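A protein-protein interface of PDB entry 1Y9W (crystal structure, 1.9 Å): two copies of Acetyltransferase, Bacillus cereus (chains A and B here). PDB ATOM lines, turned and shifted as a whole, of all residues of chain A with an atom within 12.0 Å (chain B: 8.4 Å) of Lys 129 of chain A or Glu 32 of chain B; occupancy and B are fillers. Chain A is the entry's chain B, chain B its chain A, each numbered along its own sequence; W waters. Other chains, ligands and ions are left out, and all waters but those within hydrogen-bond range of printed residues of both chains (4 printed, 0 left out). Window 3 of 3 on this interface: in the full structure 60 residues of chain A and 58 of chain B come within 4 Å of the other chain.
Water W4 lies within hydrogen-bond range of the guanidinium group (NH2) of Arg 98 of chain B (2.6 Å), the backbone carbonyl oxygen (O) of Phe 61 of chain B (2.7 Å) and a ring nitrogen (ND1) of His 127 of chain A (2.9 Å).
Water W1 bridges the backbone carbonyl oxygen (O) of Phe 61 of chain B (2.8 Å) and the backbone NH (N) of Lys 129 of chain A (2.9 Å).
Water W3 lies within hydrogen-bond range of the backbone NH of Glu 125 of chain A (2.8 Å) and the guanidinium group of Arg 139 of chain B (3.1 Å).
Water W2 bridges N of Thr 30 of chain B (3.0 Å) and NE2 of His 131 of chain A (3.4 Å).
Of the 14 printed residues of chain A, 9 touch a printed residue of chain B.
Hydrophobic or aromatic side chains of chain A that line the printed part of chain B: Phe 105, Phe 107, Val 124, His 127, Pro 128 and His 131.
Printed residues of chain B that touch a printed residue of chain A: Leu 29, Glu 32, Val 33, Phe 61, His 63, Arg 98, Leu 99 and Arg 139.
Among the printed residues, Asp or Glu carboxylates within 4 Å of a Lys or Arg side-chain nitrogen of the other chain: Asp 126 of chain A with Arg 98 of chain B and Lys 129 of chain A with Glu 32 of chain B.
NH1 of Arg 98 of chain B lies within salt-bridge range of OD2 of Asp 126 of chain A, 3.2 Å away.
The side-chain carboxylate (OE2) of Glu 32 of chain B is in salt-bridge range of the side-chain amino group (NZ) of Lys 129 of chain A.
The guanidinium group of Arg 139 of chain B lies within hydrogen-bond range of the backbone carbonyl oxygen of Glu 125 of chain A (2.7 Å).
Of the printed residues of chain A, Glu 32 of chain B touches Lys 129 (3.3 Å).
No residue of chain A comes within 4 Å of Thr 30 of chain B.
Val 33 of chain B touches two residues of chain A.
Printed residues of chain A within 4 Å of Arg 139 of chain B: Val 124 (3.8 Å) and Glu 125 (2.7 Å).
Of the printed residues of chain B, Phe 105 of chain A touches Phe 61.
Gln 133 of chain A touches none of the printed residues of chain B.
The nearest residue of chain B that does not touch Lys 129 of chain A is Phe 61 of chain B (5.1 Å).
Among the printed residues, pairs that only touch across the chains: Phe 105 of chain A with Phe 61 of chain B (3.8 Å), Phe 107 of chain A with Leu 29 of chain B (3.8 Å), Val 124 of chain A with Leu 99 of chain B (3.8 Å), Val 124 of chain A with Arg 139 of chain B (3.8 Å), His 127 of chain A with His 63 of chain B (3.5 Å), His 127 of chain A with Arg 98 of chain B (3.8 Å), His 127 of chain A with Leu 99 of chain B (3.7 Å), Pro 128 of chain A with Val 33 of chain B (3.9 Å), Pro 128 of chain A with Phe 61 of chain B (3.8 Å), Lys 129 of chain A with Val 33 of chain B (3.6 Å), Lys 129 of chain A with Arg 98 of chain B (3.2 Å) and His 131 of chain A with Leu 29 of chain B (3.3 Å).
No position is printed for both chains.
N of Val 124 of chain A lies within hydrogen-bond range of O of Gln 133 of chain A (2.8 Å).
The backbone carbonyl oxygen of Leu 29 of chain B sits close to the side-chain amino group of Lys 34 of chain B (3.1 Å).
O of His 131 of chain A sits close to N of Asp 126 of chain A, 3.0 Å away.
The backbone NH (N) of Arg 98 of chain B lies within hydrogen-bond range of the backbone carbonyl oxygen (O) of Tyr 62 of chain B, 3.1 Å away.
The side-chain carboxylate (OD1) of Asp 126 of chain A sits at hydrogen-bond distance from the backbone NH (N) of Gly 130 of chain A, at 2.8 Å.
The backbone NH (N) of Ser 132 of chain A sits close to the backbone carbonyl oxygen (O) of His 127 of chain A.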
ATOM      1  N   PHE A 105       2.748 -20.328  22.939  1.00  0.00           N
ATOM      2  CA  PHE A 105       3.297 -20.949  21.752  1.00  0.00           C
ATOM      3  C   PHE A 105       2.188 -20.864  20.708  1.00  0.00           C
ATOM      4  O   PHE A 105       1.016 -20.659  21.056  1.00  0.00           O
ATOM      5  CB  PHE A 105       3.653 -22.397  22.038  1.00  0.00           C
ATOM      6  CG  PHE A 105       4.950 -22.561  22.763  1.00  0.00           C
ATOM      7  CD1 PHE A 105       6.156 -22.416  22.088  1.00  0.00           C
ATOM      8  CD2 PHE A 105       4.971 -22.859  24.121  1.00  0.00           C
ATOM      9  CE1 PHE A 105       7.367 -22.569  22.749  1.00  0.00           C
ATOM     10  CE2 PHE A 105       6.186 -23.015  24.796  1.00  0.00           C
ATOM     11  CZ  PHE A 105       7.383 -22.869  24.108  1.00  0.00           C
ATOM     12  N   SER A 106       2.556 -21.006  19.440  1.00  0.00           N
ATOM     13  CA  SER A 106       1.597 -20.941  18.333  1.00  0.00           C
ATOM     14  C   SER A 106       0.460 -21.955  18.459  1.00  0.00           C
ATOM     15  O   SER A 106      -0.615 -21.757  17.903  1.00  0.00           O
ATOM     16  CB  SER A 106       2.330 -21.166  17.017  1.00  0.00           C
ATOM     17  OG  SER A 106       3.102 -22.349  17.105  1.00  0.00           O
ATOM     18  N   PHE A 107       0.705 -23.045  19.181  1.00  0.00           N
ATOM     19  CA  PHE A 107      -0.316 -24.066  19.377  1.00  0.00           C
ATOM     20  C   PHE A 107      -1.140 -23.829  20.645  1.00  0.00           C
ATOM     21  O   PHE A 107      -1.936 -24.687  21.040  1.00  0.00           O
ATOM     22  CB  PHE A 107       0.317 -25.469  19.405  1.00  0.00           C
ATOM     23  CG  PHE A 107       1.503 -25.594  20.326  1.00  0.00           C
ATOM     24  CD1 PHE A 107       1.327 -25.764  21.699  1.00  0.00           C
ATOM     25  CD2 PHE A 107       2.800 -25.530  19.817  1.00  0.00           C
ATOM     26  CE1 PHE A 107       2.434 -25.869  22.555  1.00  0.00           C
ATOM     27  CE2 PHE A 107       3.912 -25.632  20.658  1.00  0.00           C
ATOM     28  CZ  PHE A 107       3.726 -25.803  22.028  1.00  0.00           C
ATOM     29  N   VAL A 124       9.797 -15.757  19.283  1.00  0.00           N
ATOM     30  CA  VAL A 124      10.914 -16.675  19.127  1.00  0.00           C
ATOM     31  C   VAL A 124      10.457 -17.623  18.026  1.00  0.00           C
ATOM     32  O   VAL A 124       9.532 -18.427  18.217  1.00  0.00           O
ATOM     33  CB  VAL A 124      11.196 -17.484  20.419  1.00  0.00           C
ATOM     34  CG1 VAL A 124      12.265 -18.533  20.146  1.00  0.00           C
ATOM     35  CG2 VAL A 124      11.652 -16.548  21.535  1.00  0.00           C
ATOM     36  N   GLU A 125      11.094 -17.500  16.867  1.00  0.00           N
ATOM     37  CA  GLU A 125      10.761 -18.319  15.706  1.00  0.00           C
ATOM     38  C   GLU A 125      11.193 -19.778  15.817  1.00  0.00           C
ATOM     39  O   GLU A 125      12.163 -20.109  16.509  1.00  0.00           O
ATOM     40  CB  GLU A 125      11.404 -17.727  14.453  1.00  0.00           C
ATOM     41  CG  GLU A 125      11.056 -16.282  14.175  1.00  0.00           C
ATOM     42  CD  GLU A 125       9.593 -16.082  13.832  1.00  0.00           C
ATOM     43  OE1 GLU A 125       8.891 -17.077  13.530  1.00  0.00           O
ATOM     44  OE2 GLU A 125       9.150 -14.916  13.854  1.00  0.00           O
ATOM     45  N   ASP A 126      10.455 -20.635  15.116  1.00  0.00           N
ATOM     46  CA  ASP A 126      10.730 -22.067  15.046  1.00  0.00           C
ATOM     47  C   ASP A 126      11.164 -22.665  16.377  1.00  0.00           C
ATOM     48  O   ASP A 126      12.209 -23.313  16.468  1.00  0.00           O
ATOM     49  CB  ASP A 126      11.801 -22.326  13.970  1.00  0.00           C
ATOM     50  CG  ASP A 126      11.916 -23.802  13.590  1.00  0.00           C
ATOM     51  OD1 ASP A 126      10.898 -24.400  13.173  1.00  0.00           O
ATOM     52  OD2 ASP A 126      13.026 -24.362  13.702  1.00  0.00           O
ATOM     53  N   HIS A 127      10.352 -22.435  17.405  1.00  0.00           N
ATOM     54  CA  HIS A 127      10.611 -22.945  18.747  1.00  0.00           C
ATOM     55  C   HIS A 127       9.290 -23.303  19.422  1.00  0.00           C
ATOM     56  O   HIS A 127       8.466 -22.429  19.686  1.00  0.00           O
ATOM     57  CB  HIS A 127      11.352 -21.897  19.595  1.00  0.00           C
ATOM     58  CG  HIS A 127      11.397 -22.226  21.058  1.00  0.00           C
ATOM     59  ND1 HIS A 127      11.939 -23.399  21.542  1.00  0.00           N
ATOM     60  CD2 HIS A 127      10.927 -21.558  22.140  1.00  0.00           C
ATOM     61  CE1 HIS A 127      11.795 -23.439  22.857  1.00  0.00           C
ATOM     62  NE2 HIS A 127      11.184 -22.335  23.244  1.00  0.00           N
ATOM     63  N   PRO A 128       9.038 -24.605  19.637  1.00  0.00           N
ATOM     64  CA  PRO A 128       9.932 -25.708  19.263  1.00  0.00           C
ATOM     65  C   PRO A 128       9.873 -25.866  17.738  1.00  0.00           C
ATOM     66  O   PRO A 128       9.019 -25.254  17.082  1.00  0.00           O
ATOM     67  CB  PRO A 128       9.326 -26.900  19.997  1.00  0.00           C
ATOM     68  CG  PRO A 128       7.845 -26.583  19.982  1.00  0.00           C
ATOM     69  CD  PRO A 128       7.827 -25.105  20.317  1.00  0.00           C
ATOM     70  N   LYS A 129      10.764 -26.676  17.172  1.00  0.00           N
ATOM     71  CA  LYS A 129      10.796 -26.870  15.726  1.00  0.00           C
ATOM     72  C   LYS A 129       9.404 -27.072  15.132  1.00  0.00           C
ATOM     73  O   LYS A 129       8.653 -27.956  15.570  1.00  0.00           O
ATOM     74  CB  LYS A 129      11.676 -28.071  15.361  1.00  0.00           C
ATOM     75  CG  LYS A 129      11.739 -28.337  13.856  1.00  0.00           C
ATOM     76  CD  LYS A 129      12.450 -29.640  13.514  1.00  0.00           C
ATOM     77  CE  LYS A 129      12.499 -29.873  12.000  1.00  0.00           C
ATOM     78  NZ  LYS A 129      11.152 -30.081  11.379  1.00  0.00           N
ATOM     79  N   GLY A 130       9.071 -26.252  14.132  1.00  0.00           N
ATOM     80  CA  GLY A 130       7.780 -26.343  13.469  1.00  0.00           C
ATOM     81  C   GLY A 130       6.728 -25.445  14.088  1.00  0.00           C
ATOM     82  O   GLY A 130       5.596 -25.375  13.603  1.00  0.00           O
ATOM     83  N   HIS A 131       7.101 -24.760  15.167  1.00  0.00           N
ATOM     84  CA  HIS A 131       6.186 -23.859  15.858  1.00  0.00           C
ATOM     85  C   HIS A 131       6.907 -22.566  16.227  1.00  0.00           C
ATOM     86  O   HIS A 131       8.010 -22.306  15.749  1.00  0.00           O
ATOM     87  CB  HIS A 131       5.631 -24.537  17.115  1.00  0.00           C
ATOM     88  CG  HIS A 131       5.138 -25.930  16.875  1.00  0.00           C
ATOM     89  ND1 HIS A 131       5.989 -27.009  16.758  1.00  0.00           N
ATOM     90  CD2 HIS A 131       3.888 -26.418  16.702  1.00  0.00           C
ATOM     91  CE1 HIS A 131       5.284 -28.102  16.525  1.00  0.00           C
ATOM     92  NE2 HIS A 131       4.005 -27.771  16.487  1.00  0.00           N
ATOM     93  N   SER A 132       6.280 -21.753  17.069  1.00  0.00           N
ATOM     94  CA  SER A 132       6.883 -20.489  17.490  1.00  0.00           C
ATOM     95  C   SER A 132       6.374 -20.058  18.868  1.00  0.00           C
ATOM     96  O   SER A 132       5.314 -20.517  19.325  1.00  0.00           O
ATOM     97  CB  SER A 132       6.577 -19.395  16.457  1.00  0.00           C
ATOM     98  OG  SER A 132       5.187 -19.350  16.147  1.00  0.00           O
ATOM     99  N   GLN A 133       7.130 -19.190  19.538  1.00  0.00           N
ATOM    100  CA  GLN A 133       6.702 -18.706  20.850  1.00  0.00           C
ATOM    101  C   GLN A 133       6.444 -17.208  20.834  1.00  0.00           C
ATOM    102  O   GLN A 133       7.262 -16.428  20.349  1.00  0.00           O
ATOM    103  CB  GLN A 133       7.728 -19.030  21.928  1.00  0.00           C
ATOM    104  CG  GLN A 133       7.121 -18.931  23.316  1.00  0.00           C
ATOM    105  CD  GLN A 133       8.097 -19.272  24.415  1.00  0.00           C
ATOM    106  OE1 GLN A 133       7.705 -19.408  25.581  1.00  0.00           O
ATOM    107  NE2 GLN A 133       9.377 -19.402  24.061  1.00  0.00           N
ATOM    108  N   HIS A 134       5.301 -16.810  21.383  1.00  0.00           N
ATOM    109  CA  HIS A 134       4.918 -15.409  21.389  1.00  0.00           C
ATOM    110  C   HIS A 134       4.793 -14.801  22.787  1.00  0.00           C
ATOM    111  O   HIS A 134       4.094 -15.327  23.645  1.00  0.00           O
ATOM    112  CB  HIS A 134       3.619 -15.272  20.599  1.00  0.00           C
ATOM    113  CG  HIS A 134       3.723 -15.822  19.207  1.00  0.00           C
ATOM    114  ND1 HIS A 134       3.741 -17.175  18.943  1.00  0.00           N
ATOM    115  CD2 HIS A 134       3.913 -15.205  18.016  1.00  0.00           C
ATOM    116  CE1 HIS A 134       3.942 -17.367  17.651  1.00  0.00           C
ATOM    117  NE2 HIS A 134       4.051 -16.189  17.065  1.00  0.00           N
ATOM    118  N   LEU B  29       2.074 -32.467  19.946  1.00  0.00           N
ATOM    119  CA  LEU B  29       3.424 -32.263  19.429  1.00  0.00           C
ATOM    120  C   LEU B  29       4.065 -33.600  19.091  1.00  0.00           C
ATOM    121  O   LEU B  29       3.739 -34.627  19.692  1.00  0.00           O
ATOM    122  CB  LEU B  29       4.301 -31.535  20.453  1.00  0.00           C
ATOM    123  CG  LEU B  29       3.947 -30.079  20.752  1.00  0.00           C
ATOM    124  CD1 LEU B  29       4.890 -29.529  21.805  1.00  0.00           C
ATOM    125  CD2 LEU B  29       4.028 -29.269  19.473  1.00  0.00           C
ATOM    126  N   THR B  30       4.983 -33.580  18.132  1.00  0.00           N
ATOM    127  CA  THR B  30       5.671 -34.792  17.716  1.00  0.00           C
ATOM    128  C   THR B  30       6.868 -35.084  18.620  1.00  0.00           C
ATOM    129  O   THR B  30       7.385 -34.193  19.299  1.00  0.00           O
ATOM    130  CB  THR B  30       6.136 -34.688  16.248  1.00  0.00           C
ATOM    131  OG1 THR B  30       6.986 -33.545  16.089  1.00  0.00           O
ATOM    132  CG2 THR B  30       4.929 -34.562  15.324  1.00  0.00           C
ATOM    133  N   ASP B  31       7.298 -36.342  18.624  1.00  0.00           N
ATOM    134  CA  ASP B  31       8.413 -36.769  19.462  1.00  0.00           C
ATOM    135  C   ASP B  31       9.706 -36.071  19.086  1.00  0.00           C
ATOM    136  O   ASP B  31      10.621 -35.946  19.897  1.00  0.00           O
ATOM    137  CB  ASP B  31       8.590 -38.288  19.365  1.00  0.00           C
ATOM    138  CG  ASP B  31       7.283 -39.035  19.554  1.00  0.00           C
ATOM    139  OD1 ASP B  31       6.435 -38.572  20.348  1.00  0.00           O
ATOM    140  OD2 ASP B  31       7.104 -40.092  18.913  1.00  0.00           O
ATOM    141  N   GLU B  32       9.768 -35.615  17.847  1.00  0.00           N
ATOM    142  CA  GLU B  32      10.937 -34.924  17.342  1.00  0.00           C
ATOM    143  C   GLU B  32      11.370 -33.747  18.230  1.00  0.00           C
ATOM    144  O   GLU B  32      12.560 -33.464  18.351  1.00  0.00           O
ATOM    145  CB  GLU B  32      10.642 -34.433  15.926  1.00  0.00           C
ATOM    146  CG  GLU B  32      11.704 -33.551  15.323  1.00  0.00           C
ATOM    147  CD  GLU B  32      11.181 -32.781  14.128  1.00  0.00           C
ATOM    148  OE1 GLU B  32      10.164 -32.071  14.282  1.00  0.00           O
ATOM    149  OE2 GLU B  32      11.787 -32.885  13.039  1.00  0.00           O
ATOM    150  N   VAL B  33      10.413 -33.059  18.848  1.00  0.00           N
ATOM    151  CA  VAL B  33      10.747 -31.910  19.694  1.00  0.00           C
ATOM    152  C   VAL B  33      10.721 -32.254  21.179  1.00  0.00           C
ATOM    153  O   VAL B  33      11.071 -31.422  22.025  1.00  0.00           O
ATOM    154  CB  VAL B  33       9.769 -30.719  19.461  1.00  0.00           C
ATOM    155  CG1 VAL B  33       9.812 -30.274  18.014  1.00  0.00           C
ATOM    156  CG2 VAL B  33       8.352 -31.118  19.840  1.00  0.00           C
ATOM    157  N   LYS B  34      10.319 -33.484  21.491  1.00  0.00           N
ATOM    158  CA  LYS B  34      10.214 -33.915  22.878  1.00  0.00           C
ATOM    159  C   LYS B  34      11.511 -34.335  23.580  1.00  0.00           C
ATOM    160  O   LYS B  34      11.665 -35.481  24.022  1.00  0.00           O
ATOM    161  CB  LYS B  34       9.153 -35.018  22.995  1.00  0.00           C
ATOM    162  CG  LYS B  34       7.753 -34.529  22.610  1.00  0.00           C
ATOM    163  CD  LYS B  34       6.688 -35.606  22.757  1.00  0.00           C
ATOM    164  CE  LYS B  34       5.357 -35.111  22.217  1.00  0.00           C
ATOM    165  NZ  LYS B  34       4.282 -36.121  22.341  1.00  0.00           N
ATOM    166  N   GLN B  35      12.440 -33.388  23.682  1.00  0.00           N
ATOM    167  CA  GLN B  35      13.692 -33.628  24.378  1.00  0.00           C
ATOM    168  C   GLN B  35      13.302 -33.827  25.837  1.00  0.00           C
ATOM    169  O   GLN B  35      12.583 -33.010  26.404  1.00  0.00           O
ATOM    170  CB  GLN B  35      14.607 -32.409  24.266  1.00  0.00           C
ATOM    171  CG  GLN B  35      15.803 -32.445  25.213  1.00  0.00           C
ATOM    172  CD  GLN B  35      16.592 -31.140  25.226  1.00  0.00           C
ATOM    173  OE1 GLN B  35      16.014 -30.053  25.197  1.00  0.00           O
ATOM    174  NE2 GLN B  35      17.912 -31.243  25.291  1.00  0.00           N
ATOM    175  N   PRO B  36      13.743 -34.929  26.461  1.00  0.00           N
ATOM    176  CA  PRO B  36      13.383 -35.134  27.869  1.00  0.00           C
ATOM    177  C   PRO B  36      13.900 -33.967  28.723  1.00  0.00           C
ATOM    178  O   PRO B  36      15.084 -33.624  28.666  1.00  0.00           O
ATOM    179  CB  PRO B  36      14.047 -36.472  28.200  1.00  0.00           C
ATOM    180  CG  PRO B  36      15.205 -36.533  27.227  1.00  0.00           C
ATOM    181  CD  PRO B  36      14.595 -36.021  25.962  1.00  0.00           C
ATOM    182  N   PHE B  61      12.361 -29.238  24.582  1.00  0.00           N
ATOM    183  CA  PHE B  61      12.024 -28.759  23.239  1.00  0.00           C
ATOM    184  C   PHE B  61      13.318 -28.506  22.486  1.00  0.00           C
ATOM    185  O   PHE B  61      13.348 -27.780  21.487  1.00  0.00           O
ATOM    186  CB  PHE B  61      11.233 -27.452  23.308  1.00  0.00           C
ATOM    187  CG  PHE B  61       9.800 -27.636  23.671  1.00  0.00           C
ATOM    188  CD1 PHE B  61       9.244 -28.908  23.738  1.00  0.00           C
ATOM    189  CD2 PHE B  61       8.986 -26.532  23.894  1.00  0.00           C
ATOM    190  CE1 PHE B  61       7.895 -29.080  24.015  1.00  0.00           C
ATOM    191  CE2 PHE B  61       7.632 -26.694  24.173  1.00  0.00           C
ATOM    192  CZ  PHE B  61       7.083 -27.972  24.231  1.00  0.00           C
ATOM    193  N   TYR B  62      14.383 -29.118  22.984  1.00  0.00           N
ATOM    194  CA  TYR B  62      15.715 -28.975  22.416  1.00  0.00           C
ATOM    195  C   TYR B  62      16.235 -27.545  22.409  1.00  0.00           C
ATOM    196  O   TYR B  62      16.700 -27.030  21.390  1.00  0.00           O
ATOM    197  CB  TYR B  62      15.777 -29.595  21.020  1.00  0.00           C
ATOM    198  CG  TYR B  62      15.776 -31.103  21.096  1.00  0.00           C
ATOM    199  CD1 TYR B  62      16.824 -31.788  21.719  1.00  0.00           C
ATOM    200  CD2 TYR B  62      14.701 -31.846  20.610  1.00  0.00           C
ATOM    201  CE1 TYR B  62      16.797 -33.177  21.859  1.00  0.00           C
ATOM    202  CE2 TYR B  62      14.663 -33.238  20.744  1.00  0.00           C
ATOM    203  CZ  TYR B  62      15.710 -33.895  21.368  1.00  0.00           C
ATOM    204  OH  TYR B  62      15.671 -35.264  21.495  1.00  0.00           O
ATOM    205  N   HIS B  63      16.146 -26.910  23.574  1.00  0.00           N
ATOM    206  CA  HIS B  63      16.654 -25.561  23.750  1.00  0.00           C
ATOM    207  C   HIS B  63      17.082 -25.418  25.199  1.00  0.00           C
ATOM    208  O   HIS B  63      16.609 -26.149  26.075  1.00  0.00           O
ATOM    209  CB  HIS B  63      15.579 -24.514  23.423  1.00  0.00           C
ATOM    210  CG  HIS B  63      14.781 -24.069  24.611  1.00  0.00           C
ATOM    211  ND1 HIS B  63      14.802 -22.773  25.076  1.00  0.00           N
ATOM    212  CD2 HIS B  63      13.941 -24.747  25.427  1.00  0.00           C
ATOM    213  CE1 HIS B  63      14.007 -22.670  26.127  1.00  0.00           C
ATOM    214  NE2 HIS B  63      13.473 -23.854  26.360  1.00  0.00           N
ATOM    215  N   GLY B  96      22.109 -31.500  21.700  1.00  0.00           N
ATOM    216  CA  GLY B  96      21.181 -31.268  20.609  1.00  0.00           C
ATOM    217  C   GLY B  96      20.350 -29.999  20.690  1.00  0.00           C
ATOM    218  O   GLY B  96      19.348 -29.874  19.980  1.00  0.00           O
ATOM    219  N   ARG B  98      19.329 -26.348  19.892  1.00  0.00           N
ATOM    220  CA  ARG B  98      19.474 -25.531  18.704  1.00  0.00           C
ATOM    221  C   ARG B  98      19.354 -24.054  19.054  1.00  0.00           C
ATOM    222  O   ARG B  98      19.727 -23.175  18.269  1.00  0.00           O
ATOM    223  CB  ARG B  98      18.366 -25.913  17.719  1.00  0.00           C
ATOM    224  CG  ARG B  98      17.739 -27.292  17.995  1.00  0.00           C
ATOM    225  CD  ARG B  98      16.345 -27.381  17.410  1.00  0.00           C
ATOM    226  NE  ARG B  98      15.515 -26.298  17.925  1.00  0.00           N
ATOM    227  CZ  ARG B  98      14.498 -25.739  17.270  1.00  0.00           C
ATOM    228  NH1 ARG B  98      14.158 -26.155  16.052  1.00  0.00           N
ATOM    229  NH2 ARG B  98      13.832 -24.741  17.830  1.00  0.00           N
ATOM    230  N   LEU B  99      18.851 -23.789  20.254  1.00  0.00           N
ATOM    231  CA  LEU B  99      18.617 -22.426  20.684  1.00  0.00           C
ATOM    232  C   LEU B  99      18.831 -22.232  22.178  1.00  0.00           C
ATOM    233  O   LEU B  99      18.716 -23.177  22.962  1.00  0.00           O
ATOM    234  CB  LEU B  99      17.173 -22.066  20.319  1.00  0.00           C
ATOM    235  CG  LEU B  99      16.439 -20.903  20.983  1.00  0.00           C
ATOM    236  CD1 LEU B  99      16.894 -19.574  20.387  1.00  0.00           C
ATOM    237  CD2 LEU B  99      14.952 -21.093  20.770  1.00  0.00           C
ATOM    238  N   ARG B 139      20.972 -18.472  18.513  1.00  0.00           N
ATOM    239  CA  ARG B 139      20.729 -19.685  17.754  1.00  0.00           C
ATOM    240  C   ARG B 139      22.024 -20.475  17.725  1.00  0.00           C
ATOM    241  O   ARG B 139      23.093 -19.903  17.511  1.00  0.00           O
ATOM    242  CB  ARG B 139      20.287 -19.314  16.341  1.00  0.00           C
ATOM    243  CG  ARG B 139      19.000 -18.514  16.319  1.00  0.00           C
ATOM    244  CD  ARG B 139      17.826 -19.410  16.622  1.00  0.00           C
ATOM    245  NE  ARG B 139      16.582 -18.666  16.779  1.00  0.00           N
ATOM    246  CZ  ARG B 139      15.376 -19.226  16.749  1.00  0.00           C
ATOM    247  NH1 ARG B 139      15.257 -20.535  16.561  1.00  0.00           N
ATOM    248  NH2 ARG B 139      14.290 -18.484  16.918  1.00  0.00           N
HETATM  249  O   HOH W   1      12.248 -28.390  19.005  1.00  0.00           O
HETATM  250  O   HOH W   2       5.167 -30.992  16.581  1.00  0.00           O
HETATM  251  O   HOH W   3      13.172 -15.573  16.590  1.00  0.00           O
HETATM  252  O   HOH W   4      13.694 -25.372  20.336  1.00  0.00           O
